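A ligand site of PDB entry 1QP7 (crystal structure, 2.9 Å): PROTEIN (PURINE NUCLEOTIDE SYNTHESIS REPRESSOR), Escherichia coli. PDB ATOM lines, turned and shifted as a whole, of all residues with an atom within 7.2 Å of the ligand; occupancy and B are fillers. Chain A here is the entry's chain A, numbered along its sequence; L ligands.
The side-chain hydroxyl of Thr 191 is in hydrogen-bond range of a nitrogen (N3) of the ligand (3.0 Å).
A nitrogen (N4) of the ligand lies close to the side-chain carboxylate (OD2) of Asp 274, at 3.0 Å.
The guanidinium group (NH2) of Arg 189 is in hydrogen-bond range of an oxygen (O1) of the ligand, 3.0 Å away.
The backbone carbonyl oxygen (O) of Thr 191 lies close to the guanidinium group (NE) of Arg 195.
NH1 of Arg 195 lies within salt-bridge range of OD1 of Asp 274 (2.6 Å).
The backbone NH (N) of Gln 291 sits at hydrogen-bond distance from the backbone carbonyl oxygen (O) of Asp 274, at 3.4 Å.
The backbone NH (N) of Asp 274 is in hydrogen-bond range of the side-chain carboxylate (OD1) of Asp 247.
OH of Tyr 72 is in hydrogen-bond range of OE1 of Gln 291 (3.3 Å).
The backbone carbonyl oxygen of Gly 245 sits at hydrogen-bond distance from the guanidinium group of Arg 195.
NH1 of Arg 195 lies close to O of Tyr 273 (3.4 Å).
The backbone carbonyl oxygen (O) of Asn 190 lies within hydrogen-bond range of the backbone NH (N) of Arg 195.
Merely in contact with the ligand: Tyr 72 (3.2 Å), Phe 73 (3.5 Å), Arg 195 (3.5 Å) and Phe 220 (3.3 Å).
Hydrophobic or aromatic side chains within 4 Å of the ligand: Tyr 72, Phe 73 and Phe 220.
Seven residues have an atom within 4 Å of the ligand: Tyr 72, Phe 73, Arg 189, Thr 191, Arg 195, Phe 220 and Asp 274.
The nearest printed residue that does not touch the ligand is Ser 123 (4.1 Å).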
ATOM      1  N   THR A  66      13.395 -21.444 -11.179  1.00  0.00           N
ATOM      2  CA  THR A  66      12.328 -20.761 -11.903  1.00  0.00           C
ATOM      3  C   THR A  66      11.629 -19.809 -10.944  1.00  0.00           C
ATOM      4  O   THR A  66      11.748 -18.613 -11.022  1.00  0.00           O
ATOM      5  CB  THR A  66      11.364 -21.784 -12.465  1.00  0.00           C
ATOM      6  OG1 THR A  66      12.054 -22.593 -13.444  1.00  0.00           O
ATOM      7  CG2 THR A  66      10.250 -21.104 -13.145  1.00  0.00           C
ATOM      8  N   SER A  67      10.889 -20.373 -10.013  1.00  0.00           N
ATOM      9  CA  SER A  67      10.154 -19.650  -8.999  1.00  0.00           C
ATOM     10  C   SER A  67      10.477 -20.486  -7.747  1.00  0.00           C
ATOM     11  O   SER A  67      10.870 -21.631  -7.835  1.00  0.00           O
ATOM     12  CB  SER A  67       8.620 -19.663  -9.296  1.00  0.00           C
ATOM     13  OG  SER A  67       7.814 -19.524  -8.092  1.00  0.00           O
ATOM     14  N   ALA A  70       6.154 -21.634  -5.124  1.00  0.00           N
ATOM     15  CA  ALA A  70       5.395 -22.812  -5.512  1.00  0.00           C
ATOM     16  C   ALA A  70       5.791 -24.065  -4.736  1.00  0.00           C
ATOM     17  O   ALA A  70       6.977 -24.516  -4.757  1.00  0.00           O
ATOM     18  CB  ALA A  70       5.654 -23.056  -6.989  1.00  0.00           C
ATOM     19  N   ALA A  71       4.781 -24.646  -4.092  1.00  0.00           N
ATOM     20  CA  ALA A  71       4.984 -25.829  -3.280  1.00  0.00           C
ATOM     21  C   ALA A  71       5.995 -26.796  -3.824  1.00  0.00           C
ATOM     22  O   ALA A  71       6.983 -27.137  -3.156  1.00  0.00           O
ATOM     23  CB  ALA A  71       3.706 -26.528  -3.074  1.00  0.00           C
ATOM     24  N   TYR A  72       5.707 -27.206  -5.062  1.00  0.00           N
ATOM     25  CA  TYR A  72       6.522 -28.172  -5.709  1.00  0.00           C
ATOM     26  C   TYR A  72       7.951 -27.707  -5.637  1.00  0.00           C
ATOM     27  O   TYR A  72       8.817 -28.330  -4.986  1.00  0.00           O
ATOM     28  CB  TYR A  72       5.989 -28.315  -7.098  1.00  0.00           C
ATOM     29  CG  TYR A  72       6.774 -29.235  -7.944  1.00  0.00           C
ATOM     30  CD1 TYR A  72       7.824 -28.776  -8.641  1.00  0.00           C
ATOM     31  CD2 TYR A  72       6.457 -30.565  -8.049  1.00  0.00           C
ATOM     32  CE1 TYR A  72       8.548 -29.620  -9.452  1.00  0.00           C
ATOM     33  CE2 TYR A  72       7.214 -31.452  -8.853  1.00  0.00           C
ATOM     34  CZ  TYR A  72       8.251 -30.945  -9.549  1.00  0.00           C
ATOM     35  OH  TYR A  72       9.035 -31.710 -10.386  1.00  0.00           O
ATOM     36  N   PHE A  73       8.181 -26.553  -6.236  1.00  0.00           N
ATOM     37  CA  PHE A  73       9.497 -25.993  -6.204  1.00  0.00           C
ATOM     38  C   PHE A  73      10.022 -25.822  -4.815  1.00  0.00           C
ATOM     39  O   PHE A  73      11.124 -26.229  -4.467  1.00  0.00           O
ATOM     40  CB  PHE A  73       9.460 -24.623  -6.801  1.00  0.00           C
ATOM     41  CG  PHE A  73       9.243 -24.678  -8.237  1.00  0.00           C
ATOM     42  CD1 PHE A  73       9.665 -25.742  -8.920  1.00  0.00           C
ATOM     43  CD2 PHE A  73       8.596 -23.682  -8.889  1.00  0.00           C
ATOM     44  CE1 PHE A  73       9.460 -25.795 -10.217  1.00  0.00           C
ATOM     45  CE2 PHE A  73       8.380 -23.748 -10.225  1.00  0.00           C
ATOM     46  CZ  PHE A  73       8.796 -24.784 -10.888  1.00  0.00           C
ATOM     47  N   SER A 123      12.334 -25.157 -15.943  1.00  0.00           N
ATOM     48  CA  SER A 123      10.984 -25.334 -16.446  1.00  0.00           C
ATOM     49  C   SER A 123      10.905 -25.453 -17.944  1.00  0.00           C
ATOM     50  O   SER A 123      10.754 -26.523 -18.417  1.00  0.00           O
ATOM     51  CB  SER A 123      10.016 -24.325 -15.876  1.00  0.00           C
ATOM     52  OG  SER A 123      10.049 -24.486 -14.482  1.00  0.00           O
ATOM     53  N   ASP A 145      15.119 -30.947 -14.195  1.00  0.00           N
ATOM     54  CA  ASP A 145      13.754 -31.002 -14.718  1.00  0.00           C
ATOM     55  C   ASP A 145      13.354 -31.513 -16.115  1.00  0.00           C
ATOM     56  O   ASP A 145      12.263 -31.193 -16.614  1.00  0.00           O
ATOM     57  CB  ASP A 145      13.017 -29.729 -14.350  1.00  0.00           C
ATOM     58  CG  ASP A 145      13.722 -28.446 -14.830  1.00  0.00           C
ATOM     59  OD1 ASP A 145      14.537 -28.505 -15.795  1.00  0.00           O
ATOM     60  OD2 ASP A 145      13.359 -27.374 -14.273  1.00  0.00           O
ATOM     61  N   ASP A 159      12.387 -38.095 -14.044  1.00  0.00           N
ATOM     62  CA  ASP A 159      11.262 -38.452 -13.181  1.00  0.00           C
ATOM     63  C   ASP A 159      10.178 -39.386 -13.642  1.00  0.00           C
ATOM     64  O   ASP A 159       9.300 -39.726 -12.861  1.00  0.00           O
ATOM     65  CB  ASP A 159      10.609 -37.157 -12.730  1.00  0.00           C
ATOM     66  CG  ASP A 159       9.919 -36.424 -13.868  1.00  0.00           C
ATOM     67  OD1 ASP A 159       9.843 -37.027 -14.962  1.00  0.00           O
ATOM     68  OD2 ASP A 159       9.467 -35.265 -13.685  1.00  0.00           O
ATOM     69  N   PRO A 186       1.527 -26.517 -18.483  1.00  0.00           N
ATOM     70  CA  PRO A 186       2.196 -26.102 -19.738  1.00  0.00           C
ATOM     71  C   PRO A 186       2.926 -27.183 -20.518  1.00  0.00           C
ATOM     72  O   PRO A 186       3.854 -27.849 -20.023  1.00  0.00           O
ATOM     73  CB  PRO A 186       3.153 -25.016 -19.286  1.00  0.00           C
ATOM     74  CG  PRO A 186       2.845 -24.754 -17.845  1.00  0.00           C
ATOM     75  CD  PRO A 186       2.166 -25.957 -17.287  1.00  0.00           C
ATOM     76  N   ARG A 189       6.632 -28.095 -20.817  1.00  0.00           N
ATOM     77  CA  ARG A 189       7.282 -28.642 -19.676  1.00  0.00           C
ATOM     78  C   ARG A 189       7.112 -30.121 -19.643  1.00  0.00           C
ATOM     79  O   ARG A 189       6.189 -30.656 -20.211  1.00  0.00           O
ATOM     80  CB  ARG A 189       6.669 -28.056 -18.412  1.00  0.00           C
ATOM     81  CG  ARG A 189       7.399 -26.856 -17.940  1.00  0.00           C
ATOM     82  CD  ARG A 189       6.432 -25.788 -17.752  1.00  0.00           C
ATOM     83  NE  ARG A 189       6.439 -25.303 -16.390  1.00  0.00           N
ATOM     84  CZ  ARG A 189       6.481 -24.020 -16.130  1.00  0.00           C
ATOM     85  NH1 ARG A 189       6.499 -23.176 -17.161  1.00  0.00           N
ATOM     86  NH2 ARG A 189       6.480 -23.576 -14.878  1.00  0.00           N
ATOM     87  N   ASN A 190       8.020 -30.765 -18.945  1.00  0.00           N
ATOM     88  CA  ASN A 190       7.994 -32.197 -18.784  1.00  0.00           C
ATOM     89  C   ASN A 190       6.736 -32.558 -18.009  1.00  0.00           C
ATOM     90  O   ASN A 190       5.840 -33.274 -18.489  1.00  0.00           O
ATOM     91  CB  ASN A 190       9.216 -32.580 -17.955  1.00  0.00           C
ATOM     92  CG  ASN A 190       9.347 -34.020 -17.818  1.00  0.00           C
ATOM     93  OD1 ASN A 190       9.091 -34.757 -18.775  1.00  0.00           O
ATOM     94  ND2 ASN A 190       9.653 -34.476 -16.617  1.00  0.00           N
ATOM     95  N   THR A 191       6.709 -32.028 -16.785  1.00  0.00           N
ATOM     96  CA  THR A 191       5.631 -32.197 -15.847  1.00  0.00           C
ATOM     97  C   THR A 191       4.343 -31.834 -16.549  1.00  0.00           C
ATOM     98  O   THR A 191       3.292 -32.257 -16.094  1.00  0.00           O
ATOM     99  CB  THR A 191       5.846 -31.309 -14.636  1.00  0.00           C
ATOM    100  OG1 THR A 191       6.227 -30.012 -15.089  1.00  0.00           O
ATOM    101  CG2 THR A 191       7.024 -31.829 -13.803  1.00  0.00           C
ATOM    102  N   GLY A 192       4.427 -31.064 -17.645  1.00  0.00           N
ATOM    103  CA  GLY A 192       3.240 -30.673 -18.407  1.00  0.00           C
ATOM    104  C   GLY A 192       3.022 -31.762 -19.456  1.00  0.00           C
ATOM    105  O   GLY A 192       2.350 -32.760 -19.230  1.00  0.00           O
ATOM    106  N   ARG A 195       3.357 -35.621 -18.368  1.00  0.00           N
ATOM    107  CA  ARG A 195       2.332 -36.251 -17.572  1.00  0.00           C
ATOM    108  C   ARG A 195       1.109 -36.479 -18.447  1.00  0.00           C
ATOM    109  O   ARG A 195       0.453 -37.512 -18.394  1.00  0.00           O
ATOM    110  CB  ARG A 195       2.044 -35.356 -16.378  1.00  0.00           C
ATOM    111  CG  ARG A 195       3.196 -35.338 -15.324  1.00  0.00           C
ATOM    112  CD  ARG A 195       2.968 -34.301 -14.176  1.00  0.00           C
ATOM    113  NE  ARG A 195       4.123 -34.164 -13.304  1.00  0.00           N
ATOM    114  CZ  ARG A 195       4.121 -33.490 -12.163  1.00  0.00           C
ATOM    115  NH1 ARG A 195       3.036 -32.895 -11.721  1.00  0.00           N
ATOM    116  NH2 ARG A 195       5.229 -33.426 -11.448  1.00  0.00           N
ATOM    117  N   ASP A 219      -1.584 -23.826 -15.677  1.00  0.00           N
ATOM    118  CA  ASP A 219      -0.259 -23.201 -15.686  1.00  0.00           C
ATOM    119  C   ASP A 219       0.364 -23.542 -14.323  1.00  0.00           C
ATOM    120  O   ASP A 219       1.306 -22.927 -13.877  1.00  0.00           O
ATOM    121  CB  ASP A 219      -0.402 -21.681 -15.833  1.00  0.00           C
ATOM    122  CG  ASP A 219      -1.056 -21.043 -14.635  1.00  0.00           C
ATOM    123  OD1 ASP A 219      -1.674 -21.738 -13.804  1.00  0.00           O
ATOM    124  OD2 ASP A 219      -0.910 -19.833 -14.494  1.00  0.00           O
ATOM    125  N   PHE A 220      -0.221 -24.524 -13.664  1.00  0.00           N
ATOM    126  CA  PHE A 220       0.212 -24.989 -12.354  1.00  0.00           C
ATOM    127  C   PHE A 220      -0.253 -24.142 -11.194  1.00  0.00           C
ATOM    128  O   PHE A 220       0.031 -24.458 -10.042  1.00  0.00           O
ATOM    129  CB  PHE A 220       1.707 -25.169 -12.273  1.00  0.00           C
ATOM    130  CG  PHE A 220       2.209 -26.430 -12.901  1.00  0.00           C
ATOM    131  CD1 PHE A 220       1.845 -27.660 -12.410  1.00  0.00           C
ATOM    132  CD2 PHE A 220       3.077 -26.378 -13.991  1.00  0.00           C
ATOM    133  CE1 PHE A 220       2.312 -28.818 -12.987  1.00  0.00           C
ATOM    134  CE2 PHE A 220       3.529 -27.519 -14.576  1.00  0.00           C
ATOM    135  CZ  PHE A 220       3.155 -28.752 -14.075  1.00  0.00           C
ATOM    136  N   GLU A 221      -0.955 -23.055 -11.480  1.00  0.00           N
ATOM    137  CA  GLU A 221      -1.407 -22.203 -10.391  1.00  0.00           C
ATOM    138  C   GLU A 221      -2.886 -22.337 -10.101  1.00  0.00           C
ATOM    139  O   GLU A 221      -3.711 -22.506 -11.001  1.00  0.00           O
ATOM    140  CB  GLU A 221      -1.027 -20.734 -10.664  1.00  0.00           C
ATOM    141  CG  GLU A 221       0.494 -20.427 -10.759  1.00  0.00           C
ATOM    142  CD  GLU A 221       1.137 -20.097  -9.412  1.00  0.00           C
ATOM    143  OE1 GLU A 221       1.019 -18.925  -8.957  1.00  0.00           O
ATOM    144  OE2 GLU A 221       1.757 -21.006  -8.798  1.00  0.00           O
ATOM    145  N   GLY A 245      -3.123 -32.070 -13.626  1.00  0.00           N
ATOM    146  CA  GLY A 245      -1.667 -31.988 -13.754  1.00  0.00           C
ATOM    147  C   GLY A 245      -0.732 -31.751 -12.572  1.00  0.00           C
ATOM    148  O   GLY A 245       0.448 -32.088 -12.653  1.00  0.00           O
ATOM    149  N   GLY A 246      -1.271 -31.152 -11.495  1.00  0.00           N
ATOM    150  CA  GLY A 246      -0.522 -30.832 -10.277  1.00  0.00           C
ATOM    151  C   GLY A 246      -1.483 -30.559  -9.101  1.00  0.00           C
ATOM    152  O   GLY A 246      -2.635 -30.096  -9.253  1.00  0.00           O
ATOM    153  N   ASP A 247      -0.985 -30.838  -7.898  1.00  0.00           N
ATOM    154  CA  ASP A 247      -1.777 -30.642  -6.705  1.00  0.00           C
ATOM    155  C   ASP A 247      -2.346 -29.258  -6.443  1.00  0.00           C
ATOM    156  O   ASP A 247      -3.491 -29.125  -6.012  1.00  0.00           O
ATOM    157  CB  ASP A 247      -1.075 -31.207  -5.498  1.00  0.00           C
ATOM    158  CG  ASP A 247      -0.845 -32.708  -5.610  1.00  0.00           C
ATOM    159  OD1 ASP A 247      -1.109 -33.270  -6.698  1.00  0.00           O
ATOM    160  OD2 ASP A 247      -0.384 -33.336  -4.613  1.00  0.00           O
ATOM    161  N   ILE A 248      -1.580 -28.201  -6.707  1.00  0.00           N
ATOM    162  CA  ILE A 248      -2.119 -26.850  -6.447  1.00  0.00           C
ATOM    163  C   ILE A 248      -3.271 -26.487  -7.362  1.00  0.00           C
ATOM    164  O   ILE A 248      -4.288 -26.009  -6.884  1.00  0.00           O
ATOM    165  CB  ILE A 248      -1.128 -25.734  -6.570  1.00  0.00           C
ATOM    166  CG1 ILE A 248       0.149 -26.019  -5.757  1.00  0.00           C
ATOM    167  CG2 ILE A 248      -1.829 -24.419  -6.246  1.00  0.00           C
ATOM    168  CD1 ILE A 248      -0.121 -26.130  -4.337  1.00  0.00           C
ATOM    169  N   TYR A 273      -1.586 -34.682  -8.726  1.00  0.00           N
ATOM    170  CA  TYR A 273      -0.269 -35.026  -9.170  1.00  0.00           C
ATOM    171  C   TYR A 273       0.784 -34.175  -8.605  1.00  0.00           C
ATOM    172  O   TYR A 273       0.914 -33.021  -9.045  1.00  0.00           O
ATOM    173  CB  TYR A 273      -0.154 -34.905 -10.657  1.00  0.00           C
ATOM    174  CG  TYR A 273       0.990 -35.764 -11.133  1.00  0.00           C
ATOM    175  CD1 TYR A 273       2.216 -35.737 -10.498  1.00  0.00           C
ATOM    176  CD2 TYR A 273       0.832 -36.628 -12.198  1.00  0.00           C
ATOM    177  CE1 TYR A 273       3.240 -36.516 -10.904  1.00  0.00           C
ATOM    178  CE2 TYR A 273       1.879 -37.421 -12.627  1.00  0.00           C
ATOM    179  CZ  TYR A 273       3.090 -37.368 -11.970  1.00  0.00           C
ATOM    180  OH  TYR A 273       4.135 -38.151 -12.378  1.00  0.00           O
ATOM    181  N   ASP A 274       1.568 -34.795  -7.706  1.00  0.00           N
ATOM    182  CA  ASP A 274       2.724 -34.198  -7.018  1.00  0.00           C
ATOM    183  C   ASP A 274       2.911 -34.639  -5.586  1.00  0.00           C
ATOM    184  O   ASP A 274       4.021 -34.767  -5.110  1.00  0.00           O
ATOM    185  CB  ASP A 274       2.663 -32.659  -6.992  1.00  0.00           C
ATOM    186  CG  ASP A 274       3.276 -32.031  -8.213  1.00  0.00           C
ATOM    187  OD1 ASP A 274       3.657 -32.770  -9.166  1.00  0.00           O
ATOM    188  OD2 ASP A 274       3.294 -30.801  -8.272  1.00  0.00           O
ATOM    189  N   VAL A 276       2.074 -33.053  -2.802  1.00  0.00           N
ATOM    190  CA  VAL A 276       2.682 -31.944  -2.109  1.00  0.00           C
ATOM    191  C   VAL A 276       2.430 -32.051  -0.590  1.00  0.00           C
ATOM    192  O   VAL A 276       1.409 -32.549  -0.157  1.00  0.00           O
ATOM    193  CB  VAL A 276       2.055 -30.685  -2.644  1.00  0.00           C
ATOM    194  CG1 VAL A 276       1.714 -29.763  -1.495  1.00  0.00           C
ATOM    195  CG2 VAL A 276       2.963 -30.094  -3.700  1.00  0.00           C
ATOM    196  N   GLN A 291       5.455 -37.545  -6.314  1.00  0.00           N
ATOM    197  CA  GLN A 291       6.749 -37.342  -6.950  1.00  0.00           C
ATOM    198  C   GLN A 291       7.755 -37.230  -5.834  1.00  0.00           C
ATOM    199  O   GLN A 291       7.610 -36.384  -4.933  1.00  0.00           O
ATOM    200  CB  GLN A 291       6.846 -35.996  -7.629  1.00  0.00           C
ATOM    201  CG  GLN A 291       8.262 -35.721  -8.066  1.00  0.00           C
ATOM    202  CD  GLN A 291       8.420 -35.910  -9.564  1.00  0.00           C
ATOM    203  OE1 GLN A 291       8.774 -34.969 -10.253  1.00  0.00           O
ATOM    204  NE2 GLN A 291       8.089 -37.102 -10.090  1.00  0.00           N
HETATM  205  N1  LIG L   1       5.427 -25.485 -11.482  1.00  0.00           N
HETATM  206  C1  LIG L   1       4.754 -25.682 -10.298  1.00  0.00           C
HETATM  207  N2  LIG L   1       4.472 -26.869  -9.804  1.00  0.00           N
HETATM  208  C2  LIG L   1       4.912 -27.884 -10.600  1.00  0.00           C
HETATM  209  C3  LIG L   1       5.591 -27.789 -11.794  1.00  0.00           C
HETATM  210  C4  LIG L   1       5.888 -26.505 -12.299  1.00  0.00           C
HETATM  211  O1  LIG L   1       6.500 -26.192 -13.338  1.00  0.00           O
HETATM  212  N3  LIG L   1       5.867 -29.053 -12.292  1.00  0.00           N
HETATM  213  C5  LIG L   1       5.339 -29.878 -11.438  1.00  0.00           C
HETATM  214  N4  LIG L   1       4.756 -29.239 -10.377  1.00  0.00           N
